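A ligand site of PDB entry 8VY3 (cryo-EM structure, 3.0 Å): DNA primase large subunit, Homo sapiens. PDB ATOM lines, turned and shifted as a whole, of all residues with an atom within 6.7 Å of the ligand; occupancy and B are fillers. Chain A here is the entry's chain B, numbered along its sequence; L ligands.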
ATOM      1  N   PRO A 264      12.245  -1.312  -6.918  1.00  0.00           N
ATOM      2  CA  PRO A 264      11.298  -1.786  -5.908  1.00  0.00           C
ATOM      3  C   PRO A 264      11.680  -3.165  -5.419  1.00  0.00           C
ATOM      4  O   PRO A 264      12.551  -3.819  -6.008  1.00  0.00           O
ATOM      5  CB  PRO A 264       9.958  -1.800  -6.670  1.00  0.00           C
ATOM      6  CG  PRO A 264      10.344  -1.953  -8.081  1.00  0.00           C
ATOM      7  CD  PRO A 264      11.602  -1.154  -8.233  1.00  0.00           C
ATOM      8  N   PRO A 265      11.066  -3.653  -4.326  1.00  0.00           N
ATOM      9  CA  PRO A 265      11.467  -4.950  -3.764  1.00  0.00           C
ATOM     10  C   PRO A 265      11.388  -6.132  -4.730  1.00  0.00           C
ATOM     11  O   PRO A 265      12.254  -7.008  -4.685  1.00  0.00           O
ATOM     12  CB  PRO A 265      10.487  -5.129  -2.602  1.00  0.00           C
ATOM     13  CG  PRO A 265      10.210  -3.750  -2.160  1.00  0.00           C
ATOM     14  CD  PRO A 265      10.131  -2.949  -3.429  1.00  0.00           C
ATOM     15  N   CYS A 266      10.369  -6.177  -5.586  1.00  0.00           N
ATOM     16  CA  CYS A 266      10.207  -7.292  -6.511  1.00  0.00           C
ATOM     17  C   CYS A 266      11.388  -7.353  -7.483  1.00  0.00           C
ATOM     18  O   CYS A 266      11.989  -8.417  -7.690  1.00  0.00           O
ATOM     19  CB  CYS A 266       8.893  -7.166  -7.281  1.00  0.00           C
ATOM     20  SG  CYS A 266       8.382  -5.472  -7.680  1.00  0.00           S
ATOM     21  N   MET A 267      11.737  -6.210  -8.062  1.00  0.00           N
ATOM     22  CA  MET A 267      12.847  -6.170  -8.998  1.00  0.00           C
ATOM     23  C   MET A 267      14.177  -6.381  -8.275  1.00  0.00           C
ATOM     24  O   MET A 267      15.100  -6.959  -8.852  1.00  0.00           O
ATOM     25  CB  MET A 267      12.834  -4.854  -9.756  1.00  0.00           C
ATOM     26  CG  MET A 267      11.568  -4.671 -10.561  1.00  0.00           C
ATOM     27  SD  MET A 267      11.064  -6.188 -11.372  1.00  0.00           S
ATOM     28  CE  MET A 267       9.480  -5.714 -12.045  1.00  0.00           C
ATOM     29  N   GLN A 287       9.093 -10.813 -16.389  1.00  0.00           N
ATOM     30  CA  GLN A 287       8.893  -9.676 -15.495  1.00  0.00           C
ATOM     31  C   GLN A 287      10.099  -8.737 -15.504  1.00  0.00           C
ATOM     32  O   GLN A 287       9.968  -7.536 -15.750  1.00  0.00           O
ATOM     33  CB  GLN A 287       8.619 -10.171 -14.077  1.00  0.00           C
ATOM     34  CG  GLN A 287       8.159  -9.097 -13.118  1.00  0.00           C
ATOM     35  CD  GLN A 287       7.719  -9.682 -11.792  1.00  0.00           C
ATOM     36  OE1 GLN A 287       8.307  -9.400 -10.755  1.00  0.00           O
ATOM     37  NE2 GLN A 287       6.707 -10.528 -11.832  1.00  0.00           N
ATOM     38  N   SER A 345       2.354  -4.428 -14.627  1.00  0.00           N
ATOM     39  CA  SER A 345       1.876  -3.460 -13.656  1.00  0.00           C
ATOM     40  C   SER A 345       1.756  -4.094 -12.273  1.00  0.00           C
ATOM     41  O   SER A 345       1.844  -5.305 -12.110  1.00  0.00           O
ATOM     42  CB  SER A 345       0.536  -2.881 -14.108  1.00  0.00           C
ATOM     43  OG  SER A 345      -0.533  -3.722 -13.716  1.00  0.00           O
ATOM     44  N   CYS A 346       1.548  -3.250 -11.267  1.00  0.00           N
ATOM     45  CA  CYS A 346       1.521  -3.711  -9.887  1.00  0.00           C
ATOM     46  C   CYS A 346       0.366  -4.680  -9.652  1.00  0.00           C
ATOM     47  O   CYS A 346       0.522  -5.722  -9.004  1.00  0.00           O
ATOM     48  CB  CYS A 346       1.422  -2.501  -8.951  1.00  0.00           C
ATOM     49  SG  CYS A 346       2.210  -2.701  -7.360  1.00  0.00           S
ATOM     50  N   LEU A 347      -0.809  -4.359 -10.200  1.00  0.00           N
ATOM     51  CA  LEU A 347      -1.972  -5.218 -10.064  1.00  0.00           C
ATOM     52  C   LEU A 347      -1.783  -6.558 -10.770  1.00  0.00           C
ATOM     53  O   LEU A 347      -2.230  -7.595 -10.275  1.00  0.00           O
ATOM     54  CB  LEU A 347      -3.211  -4.505 -10.613  1.00  0.00           C
ATOM     55  CG  LEU A 347      -4.482  -4.509  -9.765  1.00  0.00           C
ATOM     56  CD1 LEU A 347      -4.175  -4.127  -8.335  1.00  0.00           C
ATOM     57  CD2 LEU A 347      -5.513  -3.583 -10.367  1.00  0.00           C
ATOM     58  N   ILE A 349       1.116  -8.095 -11.329  1.00  0.00           N
ATOM     59  CA  ILE A 349       2.085  -8.833 -10.535  1.00  0.00           C
ATOM     60  C   ILE A 349       1.383  -9.434  -9.318  1.00  0.00           C
ATOM     61  O   ILE A 349       1.609 -10.599  -8.966  1.00  0.00           O
ATOM     62  CB  ILE A 349       3.263  -7.947 -10.112  1.00  0.00           C
ATOM     63  CG1 ILE A 349       4.040  -7.490 -11.344  1.00  0.00           C
ATOM     64  CG2 ILE A 349       4.163  -8.672  -9.152  1.00  0.00           C
ATOM     65  CD1 ILE A 349       5.227  -6.622 -11.037  1.00  0.00           C
ATOM     66  N   ILE A 350       0.528  -8.641  -8.678  1.00  0.00           N
ATOM     67  CA  ILE A 350      -0.132  -9.095  -7.452  1.00  0.00           C
ATOM     68  C   ILE A 350      -1.171 -10.196  -7.700  1.00  0.00           C
ATOM     69  O   ILE A 350      -1.167 -11.213  -6.996  1.00  0.00           O
ATOM     70  CB  ILE A 350      -0.772  -7.901  -6.729  1.00  0.00           C
ATOM     71  CG1 ILE A 350       0.308  -7.025  -6.087  1.00  0.00           C
ATOM     72  CG2 ILE A 350      -1.751  -8.375  -5.679  1.00  0.00           C
ATOM     73  CD1 ILE A 350      -0.238  -5.887  -5.283  1.00  0.00           C
ATOM     74  N   GLY A 362       6.842 -12.312  -8.613  1.00  0.00           N
ATOM     75  CA  GLY A 362       5.732 -11.961  -7.760  1.00  0.00           C
ATOM     76  C   GLY A 362       6.026 -10.735  -6.920  1.00  0.00           C
ATOM     77  O   GLY A 362       7.041 -10.068  -7.054  1.00  0.00           O
ATOM     78  N   CYS A 363       5.083 -10.433  -6.030  1.00  0.00           N
ATOM     79  CA  CYS A 363       5.210  -9.287  -5.131  1.00  0.00           C
ATOM     80  C   CYS A 363       5.627  -9.765  -3.751  1.00  0.00           C
ATOM     81  O   CYS A 363       4.958 -10.640  -3.183  1.00  0.00           O
ATOM     82  CB  CYS A 363       3.903  -8.526  -5.047  1.00  0.00           C
ATOM     83  SG  CYS A 363       3.905  -7.112  -3.925  1.00  0.00           S
ATOM     84  N   PRO A 364       6.720  -9.241  -3.183  1.00  0.00           N
ATOM     85  CA  PRO A 364       7.161  -9.675  -1.858  1.00  0.00           C
ATOM     86  C   PRO A 364       6.125  -9.475  -0.758  1.00  0.00           C
ATOM     87  O   PRO A 364       6.000 -10.309   0.133  1.00  0.00           O
ATOM     88  CB  PRO A 364       8.407  -8.816  -1.602  1.00  0.00           C
ATOM     89  CG  PRO A 364       8.898  -8.493  -2.953  1.00  0.00           C
ATOM     90  CD  PRO A 364       7.677  -8.297  -3.793  1.00  0.00           C
ATOM     91  N   PHE A 365       5.380  -8.384  -0.827  1.00  0.00           N
ATOM     92  CA  PHE A 365       4.433  -8.044   0.224  1.00  0.00           C
ATOM     93  C   PHE A 365       3.222  -8.968   0.209  1.00  0.00           C
ATOM     94  O   PHE A 365       2.491  -9.059   1.204  1.00  0.00           O
ATOM     95  CB  PHE A 365       3.988  -6.594   0.099  1.00  0.00           C
ATOM     96  CG  PHE A 365       5.091  -5.600   0.308  1.00  0.00           C
ATOM     97  CD1 PHE A 365       5.646  -5.436   1.558  1.00  0.00           C
ATOM     98  CD2 PHE A 365       5.570  -4.847  -0.741  1.00  0.00           C
ATOM     99  CE1 PHE A 365       6.674  -4.524   1.756  1.00  0.00           C
ATOM    100  CE2 PHE A 365       6.584  -3.934  -0.548  1.00  0.00           C
ATOM    101  CZ  PHE A 365       7.132  -3.776   0.699  1.00  0.00           C
ATOM    102  N   ARG A 366       2.995  -9.673  -0.900  1.00  0.00           N
ATOM    103  CA  ARG A 366       1.819 -10.509  -1.062  1.00  0.00           C
ATOM    104  C   ARG A 366       2.137 -11.996  -0.969  1.00  0.00           C
ATOM    105  O   ARG A 366       1.427 -12.745  -0.287  1.00  0.00           O
ATOM    106  CB  ARG A 366       1.129 -10.192  -2.394  1.00  0.00           C
ATOM    107  CG  ARG A 366       0.312 -11.343  -2.941  1.00  0.00           C
ATOM    108  CD  ARG A 366      -1.066 -11.364  -2.355  1.00  0.00           C
ATOM    109  NE  ARG A 366      -2.079 -11.695  -3.352  1.00  0.00           N
ATOM    110  CZ  ARG A 366      -2.759 -12.823  -3.377  1.00  0.00           C
ATOM    111  NH1 ARG A 366      -2.563 -13.775  -2.483  1.00  0.00           N
ATOM    112  NH2 ARG A 366      -3.669 -13.011  -4.330  1.00  0.00           N
ATOM    113  N   TYR A 399      -1.182  -3.903   0.152  1.00  0.00           N
ATOM    114  CA  TYR A 399       0.205  -4.143  -0.228  1.00  0.00           C
ATOM    115  C   TYR A 399       0.878  -2.900  -0.801  1.00  0.00           C
ATOM    116  O   TYR A 399       2.039  -2.605  -0.479  1.00  0.00           O
ATOM    117  CB  TYR A 399       0.260  -5.293  -1.237  1.00  0.00           C
ATOM    118  CG  TYR A 399      -0.552  -6.498  -0.840  1.00  0.00           C
ATOM    119  CD1 TYR A 399      -0.240  -7.227   0.298  1.00  0.00           C
ATOM    120  CD2 TYR A 399      -1.621  -6.918  -1.602  1.00  0.00           C
ATOM    121  CE1 TYR A 399      -0.973  -8.320   0.664  1.00  0.00           C
ATOM    122  CE2 TYR A 399      -2.378  -8.018  -1.236  1.00  0.00           C
ATOM    123  CZ  TYR A 399      -2.036  -8.713  -0.106  1.00  0.00           C
ATOM    124  OH  TYR A 399      -2.780  -9.813   0.265  1.00  0.00           O
ATOM    125  N   GLN A 400       0.163  -2.170  -1.652  1.00  0.00           N
ATOM    126  CA  GLN A 400       0.777  -1.021  -2.316  1.00  0.00           C
ATOM    127  C   GLN A 400       1.008   0.126  -1.351  1.00  0.00           C
ATOM    128  O   GLN A 400       1.978   0.880  -1.514  1.00  0.00           O
ATOM    129  CB  GLN A 400      -0.086  -0.582  -3.491  1.00  0.00           C
ATOM    130  CG  GLN A 400      -0.099  -1.591  -4.634  1.00  0.00           C
ATOM    131  CD  GLN A 400      -1.205  -1.339  -5.631  1.00  0.00           C
ATOM    132  OE1 GLN A 400      -1.950  -2.243  -5.994  1.00  0.00           O
ATOM    133  NE2 GLN A 400      -1.307  -0.105  -6.092  1.00  0.00           N
ATOM    134  N   VAL A 401       0.168   0.278  -0.323  1.00  0.00           N
ATOM    135  CA  VAL A 401       0.427   1.281   0.706  1.00  0.00           C
ATOM    136  C   VAL A 401       1.659   0.895   1.515  1.00  0.00           C
ATOM    137  O   VAL A 401       2.457   1.760   1.910  1.00  0.00           O
ATOM    138  CB  VAL A 401      -0.822   1.460   1.597  1.00  0.00           C
ATOM    139  CG1 VAL A 401      -0.549   2.482   2.686  1.00  0.00           C
ATOM    140  CG2 VAL A 401      -2.001   1.880   0.756  1.00  0.00           C
ATOM    141  N   ALA A 402       1.847  -0.393   1.762  1.00  0.00           N
ATOM    142  CA  ALA A 402       3.056  -0.860   2.431  1.00  0.00           C
ATOM    143  C   ALA A 402       4.298  -0.551   1.596  1.00  0.00           C
ATOM    144  O   ALA A 402       5.332  -0.130   2.127  1.00  0.00           O
ATOM    145  CB  ALA A 402       2.956  -2.351   2.719  1.00  0.00           C
ATOM    146  N   CYS A 403       4.199  -0.760   0.275  1.00  0.00           N
ATOM    147  CA  CYS A 403       5.326  -0.424  -0.596  1.00  0.00           C
ATOM    148  C   CYS A 403       5.563   1.082  -0.621  1.00  0.00           C
ATOM    149  O   CYS A 403       6.703   1.531  -0.749  1.00  0.00           O
ATOM    150  CB  CYS A 403       5.068  -0.971  -1.997  1.00  0.00           C
ATOM    151  SG  CYS A 403       6.531  -1.104  -3.049  1.00  0.00           S
ATOM    152  N   GLN A 404       4.493   1.877  -0.514  1.00  0.00           N
ATOM    153  CA  GLN A 404       4.634   3.320  -0.407  1.00  0.00           C
ATOM    154  C   GLN A 404       5.415   3.703   0.842  1.00  0.00           C
ATOM    155  O   GLN A 404       6.288   4.570   0.814  1.00  0.00           O
ATOM    156  CB  GLN A 404       3.251   3.972  -0.377  1.00  0.00           C
ATOM    157  CG  GLN A 404       2.828   4.667  -1.660  1.00  0.00           C
ATOM    158  CD  GLN A 404       1.329   4.832  -1.738  1.00  0.00           C
ATOM    159  OE1 GLN A 404       0.756   4.790  -2.820  1.00  0.00           O
ATOM    160  NE2 GLN A 404       0.694   5.023  -0.591  1.00  0.00           N
ATOM    161  N   LEU A 420       1.105   4.702  -5.784  1.00  0.00           N
ATOM    162  CA  LEU A 420       1.928   3.742  -6.515  1.00  0.00           C
ATOM    163  C   LEU A 420       1.080   2.622  -7.096  1.00  0.00           C
ATOM    164  O   LEU A 420       0.363   1.921  -6.372  1.00  0.00           O
ATOM    165  CB  LEU A 420       3.000   3.175  -5.600  1.00  0.00           C
ATOM    166  CG  LEU A 420       3.598   1.824  -5.963  1.00  0.00           C
ATOM    167  CD1 LEU A 420       4.669   1.996  -7.011  1.00  0.00           C
ATOM    168  CD2 LEU A 420       4.153   1.168  -4.734  1.00  0.00           C
ATOM    169  N   ASN A 421       1.156   2.456  -8.409  1.00  0.00           N
ATOM    170  CA  ASN A 421       0.431   1.383  -9.079  1.00  0.00           C
ATOM    171  C   ASN A 421       1.234   0.746 -10.204  1.00  0.00           C
ATOM    172  O   ASN A 421       0.664   0.069 -11.054  1.00  0.00           O
ATOM    173  CB  ASN A 421      -0.908   1.900  -9.595  1.00  0.00           C
ATOM    174  CG  ASN A 421      -0.745   3.046 -10.576  1.00  0.00           C
ATOM    175  OD1 ASN A 421       0.352   3.528 -10.819  1.00  0.00           O
ATOM    176  ND2 ASN A 421      -1.860   3.507 -11.141  1.00  0.00           N
ATOM    177  N   HIS A 422       2.559   0.959 -10.215  1.00  0.00           N
ATOM    178  CA  HIS A 422       3.404   0.396 -11.268  1.00  0.00           C
ATOM    179  C   HIS A 422       4.867   0.457 -10.834  1.00  0.00           C
ATOM    180  O   HIS A 422       5.325   1.489 -10.339  1.00  0.00           O
ATOM    181  CB  HIS A 422       3.185   1.162 -12.573  1.00  0.00           C
ATOM    182  CG  HIS A 422       3.624   0.414 -13.796  1.00  0.00           C
ATOM    183  ND1 HIS A 422       4.931   0.096 -14.048  1.00  0.00           N
ATOM    184  CD2 HIS A 422       2.907  -0.097 -14.825  1.00  0.00           C
ATOM    185  CE1 HIS A 422       5.013  -0.563 -15.191  1.00  0.00           C
ATOM    186  NE2 HIS A 422       3.797  -0.702 -15.675  1.00  0.00           N
ATOM    187  N   PRO A 423       5.631  -0.643 -10.995  1.00  0.00           N
ATOM    188  CA  PRO A 423       7.045  -0.643 -10.582  1.00  0.00           C
ATOM    189  C   PRO A 423       7.891   0.406 -11.280  1.00  0.00           C
ATOM    190  O   PRO A 423       8.798   1.000 -10.680  1.00  0.00           O
ATOM    191  CB  PRO A 423       7.500  -2.059 -10.940  1.00  0.00           C
ATOM    192  CG  PRO A 423       6.263  -2.863 -10.932  1.00  0.00           C
ATOM    193  CD  PRO A 423       5.203  -1.966 -11.469  1.00  0.00           C
ATOM    194  N   ASN A 424       7.613   0.628 -12.562  1.00  0.00           N
ATOM    195  CA  ASN A 424       8.376   1.611 -13.327  1.00  0.00           C
ATOM    196  C   ASN A 424       8.118   3.014 -12.780  1.00  0.00           C
ATOM    197  O   ASN A 424       8.998   3.874 -12.805  1.00  0.00           O
ATOM    198  CB  ASN A 424       8.003   1.523 -14.804  1.00  0.00           C
ATOM    199  CG  ASN A 424       8.753   0.424 -15.523  1.00  0.00           C
ATOM    200  OD1 ASN A 424       8.318  -0.720 -15.533  1.00  0.00           O
ATOM    201  ND2 ASN A 424       9.868   0.767 -16.140  1.00  0.00           N
ATOM    202  N   PHE A 426       7.563   3.536  -9.583  1.00  0.00           N
ATOM    203  CA  PHE A 426       8.429   3.535  -8.401  1.00  0.00           C
ATOM    204  C   PHE A 426       9.856   3.902  -8.768  1.00  0.00           C
ATOM    205  O   PHE A 426      10.500   4.680  -8.049  1.00  0.00           O
ATOM    206  CB  PHE A 426       8.381   2.146  -7.744  1.00  0.00           C
ATOM    207  CG  PHE A 426       9.042   2.071  -6.388  1.00  0.00           C
ATOM    208  CD1 PHE A 426      10.408   2.199  -6.231  1.00  0.00           C
ATOM    209  CD2 PHE A 426       8.274   1.800  -5.270  1.00  0.00           C
ATOM    210  CE1 PHE A 426      10.994   2.101  -4.994  1.00  0.00           C
ATOM    211  CE2 PHE A 426       8.863   1.695  -4.020  1.00  0.00           C
ATOM    212  CZ  PHE A 426      10.225   1.852  -3.886  1.00  0.00           C
HETATM  213 FE1  LIG L   1       4.245  -3.224  -6.565  1.00  0.00          FE
HETATM  214 FE2  LIG L   1       4.799  -5.225  -4.789  1.00  0.00          FE
HETATM  215 FE3  LIG L   1       5.978  -2.771  -4.499  1.00  0.00          FE
HETATM  216 FE4  LIG L   1       6.712  -4.399  -6.573  1.00  0.00          FE
HETATM  217  S1  LIG L   1       7.004  -4.803  -4.346  1.00  0.00           S
HETATM  218  S2  LIG L   1       6.266  -2.171  -6.678  1.00  0.00           S
HETATM  219  S3  LIG L   1       4.715  -5.394  -7.066  1.00  0.00           S
HETATM  220  S4  LIG L   1       3.763  -3.252  -4.330  1.00  0.00           S
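SG of Cys 346 is bound to FE1 of the ligand (2.2 Å).
The side-chain sulfur (SG) of Cys 363 binds an iron atom (FE2) of the ligand, 2.3 Å away.
SG of Cys 266 binds FE4 of the ligand (2.3 Å).
An iron atom (FE3) of the ligand is bound by the side-chain sulfur (SG) of Cys 403 (2.3 Å).
Residues that only touch the ligand: Pro 264 (3.7 Å), Pro 265 (3.7 Å), Ile 349 (3.9 Å), Pro 364 (3.6 Å) and Phe 365 (3.9 Å).
Hydrophobic or aromatic side chains within 4 Å of the ligand: Pro 264, Pro 265, Ile 349, Pro 364 and Phe 365.
Nine residues have an atom within 4 Å of the ligand: Pro 264, Pro 265, Cys 266, Cys 346, Ile 349, Cys 363, Pro 364, Phe 365 and Cys 403.
The nearest printed residue that does not touch the ligand is Gln 400 (4.2 Å).
The backbone NH (N) of Cys 346 lies close to the backbone carbonyl oxygen (O) of Asn 421, at 3.4 Å.
The side-chain sulfur of Cys 363 lies close to the backbone NH of Phe 365.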
